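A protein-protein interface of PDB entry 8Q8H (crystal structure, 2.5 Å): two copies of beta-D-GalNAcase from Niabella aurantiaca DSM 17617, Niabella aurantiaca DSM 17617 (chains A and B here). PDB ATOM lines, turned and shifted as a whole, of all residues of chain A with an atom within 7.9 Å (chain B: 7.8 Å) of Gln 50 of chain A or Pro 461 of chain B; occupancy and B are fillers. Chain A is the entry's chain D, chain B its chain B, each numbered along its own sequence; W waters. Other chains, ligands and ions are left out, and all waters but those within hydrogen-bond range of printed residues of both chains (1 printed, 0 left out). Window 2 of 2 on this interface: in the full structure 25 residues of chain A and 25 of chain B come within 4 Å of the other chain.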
ATOM      1  N   MET A   4      33.574 -17.987 -14.457  1.00  0.00           N
ATOM      2  CA  MET A   4      33.244 -19.410 -14.488  1.00  0.00           C
ATOM      3  C   MET A   4      34.099 -20.144 -13.475  1.00  0.00           C
ATOM      4  O   MET A   4      35.308 -20.138 -13.606  1.00  0.00           O
ATOM      5  CB  MET A   4      33.478 -19.990 -15.891  1.00  0.00           C
ATOM      6  CG  MET A   4      33.283 -21.496 -16.005  1.00  0.00           C
ATOM      7  SD  MET A   4      31.585 -21.999 -15.915  1.00  0.00           S
ATOM      8  CE  MET A   4      31.109 -21.558 -17.588  1.00  0.00           C
ATOM      9  N   SER A  45      28.709 -21.339 -13.641  1.00  0.00           N
ATOM     10  CA  SER A  45      28.807 -20.071 -14.338  1.00  0.00           C
ATOM     11  C   SER A  45      28.332 -18.931 -13.462  1.00  0.00           C
ATOM     12  O   SER A  45      27.242 -18.981 -12.911  1.00  0.00           O
ATOM     13  CB  SER A  45      27.961 -20.112 -15.605  1.00  0.00           C
ATOM     14  OG  SER A  45      28.018 -18.891 -16.301  1.00  0.00           O
ATOM     15  N   MET A  47      27.829 -15.890 -14.838  1.00  0.00           N
ATOM     16  CA  MET A  47      27.533 -14.956 -15.925  1.00  0.00           C
ATOM     17  C   MET A  47      26.030 -14.910 -16.210  1.00  0.00           C
ATOM     18  O   MET A  47      25.391 -15.963 -16.281  1.00  0.00           O
ATOM     19  CB  MET A  47      28.266 -15.389 -17.216  1.00  0.00           C
ATOM     20  CG  MET A  47      29.828 -15.198 -17.285  1.00  0.00           C
ATOM     21  SD  MET A  47      30.700 -16.208 -18.567  1.00  0.00           S
ATOM     22  CE  MET A  47      29.729 -15.706 -20.002  1.00  0.00           C
ATOM     23  N   LYS A  48      25.495 -13.689 -16.453  1.00  0.00           N
ATOM     24  CA  LYS A  48      24.103 -13.485 -16.871  1.00  0.00           C
ATOM     25  C   LYS A  48      23.745 -14.283 -18.111  1.00  0.00           C
ATOM     26  O   LYS A  48      22.570 -14.622 -18.321  1.00  0.00           O
ATOM     27  CB  LYS A  48      23.832 -12.021 -17.264  1.00  0.00           C
ATOM     28  CG  LYS A  48      23.668 -11.008 -16.189  1.00  0.00           C
ATOM     29  CD  LYS A  48      23.467  -9.566 -16.786  1.00  0.00           C
ATOM     30  CE  LYS A  48      24.750  -8.953 -17.238  1.00  0.00           C
ATOM     31  NZ  LYS A  48      25.742  -8.775 -16.069  1.00  0.00           N
ATOM     32  N   ASP A  49      24.712 -14.464 -19.009  1.00  0.00           N
ATOM     33  CA  ASP A  49      24.461 -15.021 -20.328  1.00  0.00           C
ATOM     34  C   ASP A  49      24.900 -16.475 -20.350  1.00  0.00           C
ATOM     35  O   ASP A  49      25.882 -16.845 -19.719  1.00  0.00           O
ATOM     36  CB  ASP A  49      25.176 -14.179 -21.392  1.00  0.00           C
ATOM     37  CG  ASP A  49      24.444 -12.809 -21.693  1.00  0.00           C
ATOM     38  OD1 ASP A  49      23.183 -12.741 -21.736  1.00  0.00           O
ATOM     39  OD2 ASP A  49      25.129 -11.779 -21.869  1.00  0.00           O
ATOM     40  N   GLN A  50      24.115 -17.316 -20.996  1.00  0.00           N
ATOM     41  CA  GLN A  50      24.450 -18.726 -21.005  1.00  0.00           C
ATOM     42  C   GLN A  50      25.581 -19.006 -21.996  1.00  0.00           C
ATOM     43  O   GLN A  50      25.824 -18.247 -22.938  1.00  0.00           O
ATOM     44  CB  GLN A  50      23.241 -19.572 -21.350  1.00  0.00           C
ATOM     45  CG  GLN A  50      22.848 -19.544 -22.792  1.00  0.00           C
ATOM     46  CD  GLN A  50      21.588 -20.403 -23.126  1.00  0.00           C
ATOM     47  OE1 GLN A  50      20.925 -20.991 -22.249  1.00  0.00           O
ATOM     48  NE2 GLN A  50      21.297 -20.498 -24.401  1.00  0.00           N
ATOM     49  N   THR A  51      26.262 -20.128 -21.790  1.00  0.00           N
ATOM     50  CA  THR A  51      27.437 -20.426 -22.605  1.00  0.00           C
ATOM     51  C   THR A  51      27.540 -21.938 -22.769  1.00  0.00           C
ATOM     52  O   THR A  51      26.711 -22.677 -22.261  1.00  0.00           O
ATOM     53  CB  THR A  51      28.679 -19.783 -21.970  1.00  0.00           C
ATOM     54  OG1 THR A  51      29.808 -19.900 -22.839  1.00  0.00           O
ATOM     55  CG2 THR A  51      29.012 -20.409 -20.638  1.00  0.00           C
ATOM     56  N   HIS A  52      28.472 -22.398 -23.594  1.00  0.00           N
ATOM     57  CA  HIS A  52      28.753 -23.831 -23.703  1.00  0.00           C
ATOM     58  C   HIS A  52      29.965 -24.227 -22.847  1.00  0.00           C
ATOM     59  O   HIS A  52      30.839 -23.412 -22.541  1.00  0.00           O
ATOM     60  CB  HIS A  52      28.998 -24.244 -25.154  1.00  0.00           C
ATOM     61  CG  HIS A  52      27.811 -24.050 -26.043  1.00  0.00           C
ATOM     62  ND1 HIS A  52      27.598 -22.887 -26.759  1.00  0.00           N
ATOM     63  CD2 HIS A  52      26.772 -24.867 -26.332  1.00  0.00           C
ATOM     64  CE1 HIS A  52      26.480 -22.997 -27.454  1.00  0.00           C
ATOM     65  NE2 HIS A  52      25.958 -24.188 -27.212  1.00  0.00           N
ATOM     66  N   ILE A  53      30.008 -25.485 -22.442  1.00  0.00           N
ATOM     67  CA  ILE A  53      31.163 -25.983 -21.716  1.00  0.00           C
ATOM     68  C   ILE A  53      31.408 -27.440 -22.109  1.00  0.00           C
ATOM     69  O   ILE A  53      30.461 -28.205 -22.350  1.00  0.00           O
ATOM     70  CB  ILE A  53      31.009 -25.784 -20.186  1.00  0.00           C
ATOM     71  CG1 ILE A  53      32.393 -25.985 -19.529  1.00  0.00           C
ATOM     72  CG2 ILE A  53      29.911 -26.687 -19.595  1.00  0.00           C
ATOM     73  CD1 ILE A  53      32.507 -25.484 -18.083  1.00  0.00           C
ATOM     74  N   GLU A 108      25.180 -26.901 -22.231  1.00  0.00           N
ATOM     75  CA  GLU A 108      25.007 -25.474 -22.013  1.00  0.00           C
ATOM     76  C   GLU A 108      25.116 -25.203 -20.517  1.00  0.00           C
ATOM     77  O   GLU A 108      24.468 -25.883 -19.725  1.00  0.00           O
ATOM     78  CB  GLU A 108      23.652 -25.013 -22.546  1.00  0.00           C
ATOM     79  CG  GLU A 108      23.551 -23.512 -22.785  1.00  0.00           C
ATOM     80  CD  GLU A 108      24.204 -23.092 -24.126  1.00  0.00           C
ATOM     81  OE1 GLU A 108      24.225 -23.940 -25.055  1.00  0.00           O
ATOM     82  OE2 GLU A 108      24.694 -21.938 -24.251  1.00  0.00           O
ATOM     83  N   ALA A 109      25.994 -24.271 -20.140  1.00  0.00           N
ATOM     84  CA  ALA A 109      26.076 -23.742 -18.784  1.00  0.00           C
ATOM     85  C   ALA A 109      25.083 -22.617 -18.571  1.00  0.00           C
ATOM     86  O   ALA A 109      25.084 -21.611 -19.304  1.00  0.00           O
ATOM     87  CB  ALA A 109      27.468 -23.211 -18.493  1.00  0.00           C
ATOM     88  N   HIS A 110      24.293 -22.762 -17.551  1.00  0.00           N
ATOM     89  CA  HIS A 110      23.234 -21.820 -17.256  1.00  0.00           C
ATOM     90  C   HIS A 110      23.606 -20.872 -16.121  1.00  0.00           C
ATOM     91  O   HIS A 110      24.405 -21.209 -15.247  1.00  0.00           O
ATOM     92  CB  HIS A 110      21.978 -22.573 -16.876  1.00  0.00           C
ATOM     93  CG  HIS A 110      21.543 -23.563 -17.897  1.00  0.00           C
ATOM     94  ND1 HIS A 110      20.940 -23.172 -19.078  1.00  0.00           N
ATOM     95  CD2 HIS A 110      21.499 -24.916 -17.861  1.00  0.00           C
ATOM     96  CE1 HIS A 110      20.629 -24.257 -19.768  1.00  0.00           C
ATOM     97  NE2 HIS A 110      20.947 -25.324 -19.045  1.00  0.00           N
ATOM     98  N   PRO A 111      22.996 -19.692 -16.058  1.00  0.00           N
ATOM     99  CA  PRO A 111      23.401 -18.724 -15.028  1.00  0.00           C
ATOM    100  C   PRO A 111      23.217 -19.262 -13.611  1.00  0.00           C
ATOM    101  O   PRO A 111      22.146 -19.768 -13.247  1.00  0.00           O
ATOM    102  CB  PRO A 111      22.499 -17.511 -15.308  1.00  0.00           C
ATOM    103  CG  PRO A 111      22.138 -17.618 -16.766  1.00  0.00           C
ATOM    104  CD  PRO A 111      22.000 -19.111 -16.990  1.00  0.00           C
ATOM    105  N   GLN A 141      33.207 -20.395 -23.250  1.00  0.00           N
ATOM    106  CA  GLN A 141      33.316 -19.085 -23.875  1.00  0.00           C
ATOM    107  C   GLN A 141      32.829 -18.011 -22.919  1.00  0.00           C
ATOM    108  O   GLN A 141      31.832 -18.196 -22.221  1.00  0.00           O
ATOM    109  CB  GLN A 141      32.506 -19.009 -25.185  1.00  0.00           C
ATOM    110  CG  GLN A 141      33.046 -19.931 -26.289  1.00  0.00           C
ATOM    111  CD  GLN A 141      32.624 -21.415 -26.110  1.00  0.00           C
ATOM    112  OE1 GLN A 141      31.585 -21.718 -25.498  1.00  0.00           O
ATOM    113  NE2 GLN A 141      33.468 -22.341 -26.601  1.00  0.00           N
ATOM    114  N   GLU A 142      33.522 -16.876 -22.930  1.00  0.00           N
ATOM    115  CA  GLU A 142      33.075 -15.645 -22.290  1.00  0.00           C
ATOM    116  C   GLU A 142      33.014 -14.629 -23.412  1.00  0.00           C
ATOM    117  O   GLU A 142      34.056 -14.271 -23.979  1.00  0.00           O
ATOM    118  CB  GLU A 142      34.027 -15.198 -21.203  1.00  0.00           C
ATOM    119  CG  GLU A 142      34.168 -16.208 -20.140  1.00  0.00           C
ATOM    120  CD  GLU A 142      35.111 -15.747 -19.060  1.00  0.00           C
ATOM    121  OE1 GLU A 142      35.667 -14.618 -19.212  1.00  0.00           O
ATOM    122  OE2 GLU A 142      35.309 -16.520 -18.079  1.00  0.00           O
ATOM    123  N   GLY A 143      31.805 -14.237 -23.785  1.00  0.00           N
ATOM    124  CA  GLY A 143      31.629 -13.474 -25.007  1.00  0.00           C
ATOM    125  C   GLY A 143      32.162 -14.260 -26.172  1.00  0.00           C
ATOM    126  O   GLY A 143      31.681 -15.355 -26.497  1.00  0.00           O
ATOM    127  N   HIS B  77      15.809 -23.439 -14.605  1.00  0.00           N
ATOM    128  CA  HIS B  77      16.963 -22.564 -14.693  1.00  0.00           C
ATOM    129  C   HIS B  77      16.516 -21.176 -14.297  1.00  0.00           C
ATOM    130  O   HIS B  77      15.325 -20.862 -14.349  1.00  0.00           O
ATOM    131  CB  HIS B  77      17.540 -22.536 -16.121  1.00  0.00           C
ATOM    132  CG  HIS B  77      17.778 -23.894 -16.691  1.00  0.00           C
ATOM    133  ND1 HIS B  77      18.745 -24.746 -16.208  1.00  0.00           N
ATOM    134  CD2 HIS B  77      17.145 -24.559 -17.683  1.00  0.00           C
ATOM    135  CE1 HIS B  77      18.702 -25.875 -16.889  1.00  0.00           C
ATOM    136  NE2 HIS B  77      17.746 -25.787 -17.792  1.00  0.00           N
ATOM    137  N   PHE B  78      17.474 -20.342 -13.898  1.00  0.00           N
ATOM    138  CA  PHE B  78      17.179 -18.928 -13.869  1.00  0.00           C
ATOM    139  C   PHE B  78      17.030 -18.426 -15.297  1.00  0.00           C
ATOM    140  O   PHE B  78      17.658 -18.937 -16.230  1.00  0.00           O
ATOM    141  CB  PHE B  78      18.281 -18.122 -13.213  1.00  0.00           C
ATOM    142  CG  PHE B  78      18.349 -18.221 -11.732  1.00  0.00           C
ATOM    143  CD1 PHE B  78      17.403 -17.596 -10.956  1.00  0.00           C
ATOM    144  CD2 PHE B  78      19.448 -18.806 -11.120  1.00  0.00           C
ATOM    145  CE1 PHE B  78      17.479 -17.642  -9.597  1.00  0.00           C
ATOM    146  CE2 PHE B  78      19.557 -18.858  -9.769  1.00  0.00           C
ATOM    147  CZ  PHE B  78      18.585 -18.281  -8.990  1.00  0.00           C
ATOM    148  N   ASN B  79      16.245 -17.367 -15.443  1.00  0.00           N
ATOM    149  CA  ASN B  79      16.209 -16.628 -16.691  1.00  0.00           C
ATOM    150  C   ASN B  79      17.551 -15.939 -16.943  1.00  0.00           C
ATOM    151  O   ASN B  79      18.260 -15.564 -16.013  1.00  0.00           O
ATOM    152  CB  ASN B  79      15.085 -15.612 -16.643  1.00  0.00           C
ATOM    153  CG  ASN B  79      13.773 -16.243 -16.858  1.00  0.00           C
ATOM    154  OD1 ASN B  79      13.628 -17.079 -17.746  1.00  0.00           O
ATOM    155  ND2 ASN B  79      12.795 -15.872 -16.059  1.00  0.00           N
ATOM    156  N   THR B  80      17.915 -15.829 -18.218  1.00  0.00           N
ATOM    157  CA  THR B  80      19.174 -15.218 -18.598  1.00  0.00           C
ATOM    158  C   THR B  80      19.061 -13.699 -18.662  1.00  0.00           C
ATOM    159  O   THR B  80      17.978 -13.125 -18.824  1.00  0.00           O
ATOM    160  CB  THR B  80      19.625 -15.738 -19.948  1.00  0.00           C
ATOM    161  OG1 THR B  80      18.589 -15.505 -20.885  1.00  0.00           O
ATOM    162  CG2 THR B  80      19.888 -17.222 -19.919  1.00  0.00           C
ATOM    163  N   ASP B  81      20.232 -13.054 -18.639  1.00  0.00           N
ATOM    164  CA  ASP B  81      20.344 -11.599 -18.667  1.00  0.00           C
ATOM    165  C   ASP B  81      19.643 -10.966 -17.468  1.00  0.00           C
ATOM    166  O   ASP B  81      19.008  -9.915 -17.572  1.00  0.00           O
ATOM    167  CB  ASP B  81      19.825 -11.031 -19.987  1.00  0.00           C
ATOM    168  CG  ASP B  81      20.077  -9.542 -20.116  1.00  0.00           C
ATOM    169  OD1 ASP B  81      21.252  -9.152 -19.909  1.00  0.00           O
ATOM    170  OD2 ASP B  81      19.148  -8.786 -20.505  1.00  0.00           O
ATOM    171  N   THR B 399       9.045 -10.766 -22.673  1.00  0.00           N
ATOM    172  CA  THR B 399      10.234 -11.485 -22.205  1.00  0.00           C
ATOM    173  C   THR B 399      11.331 -10.534 -21.787  1.00  0.00           C
ATOM    174  O   THR B 399      12.201 -10.904 -20.995  1.00  0.00           O
ATOM    175  CB  THR B 399      10.835 -12.416 -23.266  1.00  0.00           C
ATOM    176  OG1 THR B 399      11.043 -11.688 -24.480  1.00  0.00           O
ATOM    177  CG2 THR B 399       9.975 -13.539 -23.538  1.00  0.00           C
ATOM    178  N   ARG B 402      15.201  -6.989 -19.403  1.00  0.00           N
ATOM    179  CA  ARG B 402      15.434  -7.657 -18.125  1.00  0.00           C
ATOM    180  C   ARG B 402      16.463  -6.927 -17.257  1.00  0.00           C
ATOM    181  O   ARG B 402      16.477  -5.690 -17.165  1.00  0.00           O
ATOM    182  CB  ARG B 402      15.856  -9.106 -18.384  1.00  0.00           C
ATOM    183  CG  ARG B 402      14.811  -9.907 -19.192  1.00  0.00           C
ATOM    184  CD  ARG B 402      15.240 -11.337 -19.402  1.00  0.00           C
ATOM    185  NE  ARG B 402      14.450 -11.982 -20.437  1.00  0.00           N
ATOM    186  CZ  ARG B 402      14.756 -13.150 -20.988  1.00  0.00           C
ATOM    187  NH1 ARG B 402      15.844 -13.813 -20.625  1.00  0.00           N
ATOM    188  NH2 ARG B 402      13.958 -13.659 -21.939  1.00  0.00           N
ATOM    189  N   ALA B 456       7.743 -21.388 -19.854  1.00  0.00           N
ATOM    190  CA  ALA B 456       8.206 -20.513 -20.925  1.00  0.00           C
ATOM    191  C   ALA B 456       7.719 -20.985 -22.291  1.00  0.00           C
ATOM    192  O   ALA B 456       8.388 -20.774 -23.305  1.00  0.00           O
ATOM    193  CB  ALA B 456       9.729 -20.405 -20.928  1.00  0.00           C
ATOM    194  N   TYR B 458       7.825 -23.577 -23.711  1.00  0.00           N
ATOM    195  CA  TYR B 458       8.805 -24.486 -24.282  1.00  0.00           C
ATOM    196  C   TYR B 458       9.845 -23.759 -25.109  1.00  0.00           C
ATOM    197  O   TYR B 458      10.472 -24.362 -25.971  1.00  0.00           O
ATOM    198  CB  TYR B 458       8.118 -25.569 -25.117  1.00  0.00           C
ATOM    199  CG  TYR B 458       7.229 -26.472 -24.307  1.00  0.00           C
ATOM    200  CD1 TYR B 458       7.752 -27.515 -23.564  1.00  0.00           C
ATOM    201  CD2 TYR B 458       5.867 -26.269 -24.263  1.00  0.00           C
ATOM    202  CE1 TYR B 458       6.936 -28.346 -22.815  1.00  0.00           C
ATOM    203  CE2 TYR B 458       5.046 -27.097 -23.496  1.00  0.00           C
ATOM    204  CZ  TYR B 458       5.604 -28.123 -22.794  1.00  0.00           C
ATOM    205  OH  TYR B 458       4.821 -28.944 -22.046  1.00  0.00           O
ATOM    206  N   ALA B 459      10.049 -22.467 -24.859  1.00  0.00           N
ATOM    207  CA  ALA B 459      10.925 -21.641 -25.676  1.00  0.00           C
ATOM    208  C   ALA B 459      11.993 -20.944 -24.825  1.00  0.00           C
ATOM    209  O   ALA B 459      12.504 -19.886 -25.213  1.00  0.00           O
ATOM    210  CB  ALA B 459      10.114 -20.610 -26.479  1.00  0.00           C
ATOM    211  N   TYR B 460      12.352 -21.500 -23.659  1.00  0.00           N
ATOM    212  CA  TYR B 460      13.426 -20.865 -22.908  1.00  0.00           C
ATOM    213  C   TYR B 460      14.752 -21.104 -23.608  1.00  0.00           C
ATOM    214  O   TYR B 460      14.940 -22.158 -24.232  1.00  0.00           O
ATOM    215  CB  TYR B 460      13.425 -21.294 -21.431  1.00  0.00           C
ATOM    216  CG  TYR B 460      14.691 -21.180 -20.606  1.00  0.00           C
ATOM    217  CD1 TYR B 460      15.908 -21.642 -21.022  1.00  0.00           C
ATOM    218  CD2 TYR B 460      14.729 -20.195 -19.615  1.00  0.00           C
ATOM    219  CE1 TYR B 460      17.070 -21.440 -20.255  1.00  0.00           C
ATOM    220  CE2 TYR B 460      15.874 -19.938 -18.877  1.00  0.00           C
ATOM    221  CZ  TYR B 460      17.050 -20.552 -19.214  1.00  0.00           C
ATOM    222  OH  TYR B 460      18.188 -20.279 -18.495  1.00  0.00           O
ATOM    223  N   PRO B 461      15.667 -20.111 -23.575  1.00  0.00           N
ATOM    224  CA  PRO B 461      15.553 -18.866 -22.805  1.00  0.00           C
ATOM    225  C   PRO B 461      14.966 -17.628 -23.508  1.00  0.00           C
ATOM    226  O   PRO B 461      14.786 -16.573 -22.858  1.00  0.00           O
ATOM    227  CB  PRO B 461      17.007 -18.563 -22.479  1.00  0.00           C
ATOM    228  CG  PRO B 461      17.702 -19.056 -23.661  1.00  0.00           C
ATOM    229  CD  PRO B 461      17.030 -20.281 -24.085  1.00  0.00           C
ATOM    230  N   GLY B 462      14.730 -17.727 -24.814  1.00  0.00           N
ATOM    231  CA  GLY B 462      14.115 -16.614 -25.523  1.00  0.00           C
ATOM    232  C   GLY B 462      12.821 -16.150 -24.875  1.00  0.00           C
ATOM    233  O   GLY B 462      12.596 -14.951 -24.690  1.00  0.00           O
ATOM    234  N   ILE B 463      11.965 -17.095 -24.502  1.00  0.00           N
ATOM    235  CA  ILE B 463      10.818 -16.816 -23.651  1.00  0.00           C
ATOM    236  C   ILE B 463      11.233 -17.061 -22.206  1.00  0.00           C
ATOM    237  O   ILE B 463      11.606 -18.184 -21.851  1.00  0.00           O
ATOM    238  CB  ILE B 463       9.622 -17.710 -24.018  1.00  0.00           C
ATOM    239  CG1 ILE B 463       9.175 -17.471 -25.469  1.00  0.00           C
ATOM    240  CG2 ILE B 463       8.514 -17.506 -23.013  1.00  0.00           C
ATOM    241  CD1 ILE B 463       8.899 -15.991 -25.794  1.00  0.00           C
ATOM    242  N   ALA B 464      11.113 -16.040 -21.358  1.00  0.00           N
ATOM    243  CA  ALA B 464      11.452 -16.178 -19.947  1.00  0.00           C
ATOM    244  C   ALA B 464      10.351 -16.889 -19.190  1.00  0.00           C
ATOM    245  O   ALA B 464       9.166 -16.583 -19.355  1.00  0.00           O
ATOM    246  CB  ALA B 464      11.681 -14.808 -19.310  1.00  0.00           C
ATOM    247  N   TYR B 465      10.755 -17.768 -18.290  1.00  0.00           N
ATOM    248  CA  TYR B 465       9.808 -18.348 -17.361  1.00  0.00           C
ATOM    249  C   TYR B 465       9.000 -17.260 -16.687  1.00  0.00           C
ATOM    250  O   TYR B 465       9.546 -16.306 -16.138  1.00  0.00           O
ATOM    251  CB  TYR B 465      10.536 -19.151 -16.302  1.00  0.00           C
ATOM    252  CG  TYR B 465      11.261 -20.339 -16.856  1.00  0.00           C
ATOM    253  CD1 TYR B 465      10.563 -21.410 -17.428  1.00  0.00           C
ATOM    254  CD2 TYR B 465      12.638 -20.441 -16.752  1.00  0.00           C
ATOM    255  CE1 TYR B 465      11.251 -22.512 -17.941  1.00  0.00           C
ATOM    256  CE2 TYR B 465      13.317 -21.570 -17.242  1.00  0.00           C
ATOM    257  CZ  TYR B 465      12.629 -22.568 -17.832  1.00  0.00           C
ATOM    258  OH  TYR B 465      13.305 -23.639 -18.292  1.00  0.00           O
HETATM  259  O   HOH W   1      20.175 -21.344 -14.340  1.00  0.00           O
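No position is printed for both chains. Of the 6 pairs that touch across the chains among the printed residues, none has its exchanged pair printed and touching as well.
The backbone carbonyl oxygen (O) of Thr 80 of chain B sits at hydrogen-bond distance from the guanidinium group (NH1) of Arg 402 of chain B (2.9 Å). The side-chain hydroxyl (OH) of Tyr 460 of chain B lies within hydrogen-bond range of the backbone carbonyl oxygen (O) of Phe 78 of chain B, at 2.7 Å. The guanidinium group of Arg 402 of chain B sits at hydrogen-bond distance from the backbone carbonyl oxygen of Pro 461 of chain B (3.2 Å).
N of Asp 81 of chain B lies within hydrogen-bond range of O of Lys 48 of chain A. A ring nitrogen (NE2) of His 77 of chain B lies close to a ring nitrogen (NE2) of His 110 of chain A (3.5 Å).
Printed residues of chain B that touch a printed residue of chain A: His 77, Phe 78, Thr 80, Asp 81 and Pro 461. Hydrophobic or aromatic side chains of chain B that line the printed part of chain A: His 77, Phe 78 and Pro 461. Hydrophobic or aromatic side chains of chain A that line the printed part of chain B: His 110 and Pro 111. Among the printed residues, 6 pairs touch across the chains. Among the printed residues, no Asp or Glu carboxylate lies within 4 Å of a Lys or Arg side-chain nitrogen of the other chain.
Water W1 lies within hydrogen-bond range of O of Pro 111 of chain A (2.8 Å) and N of Phe 78 of chain B (2.9 Å).
Of chain B, only Pro 461 (3.9 Å) comes within 4 Å of Gln 50 of chain A. Of the printed residues of chain B, Pro 111 of chain A touches Phe 78 (3.6 Å) and Thr 80 (3.9 Å). Of the printed residues of chain A, His 77 of chain B touches His 110. Pro 461 of chain B touches just one residue of chain A: Gln 50. No residue of chain A comes within 4 Å of Gly 462 of chain B. The nearest printed residue of chain B that does not touch Gln 50 of chain A is Thr 80 of chain B (4.3 Å). The nearest residue of chain A that does not touch Pro 461 of chain B is His 110 of chain A (6.9 Å).
Among the printed residues, merely in contact across the chains: Lys 48 of chain A with Thr 80 of chain B (3.5 Å), Gln 50 of chain A with Pro 461 of chain B (3.9 Å), Pro 111 of chain A with Phe 78 of chain B (3.6 Å) and Pro 111 of chain A with Thr 80 of chain B (3.9 Å).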
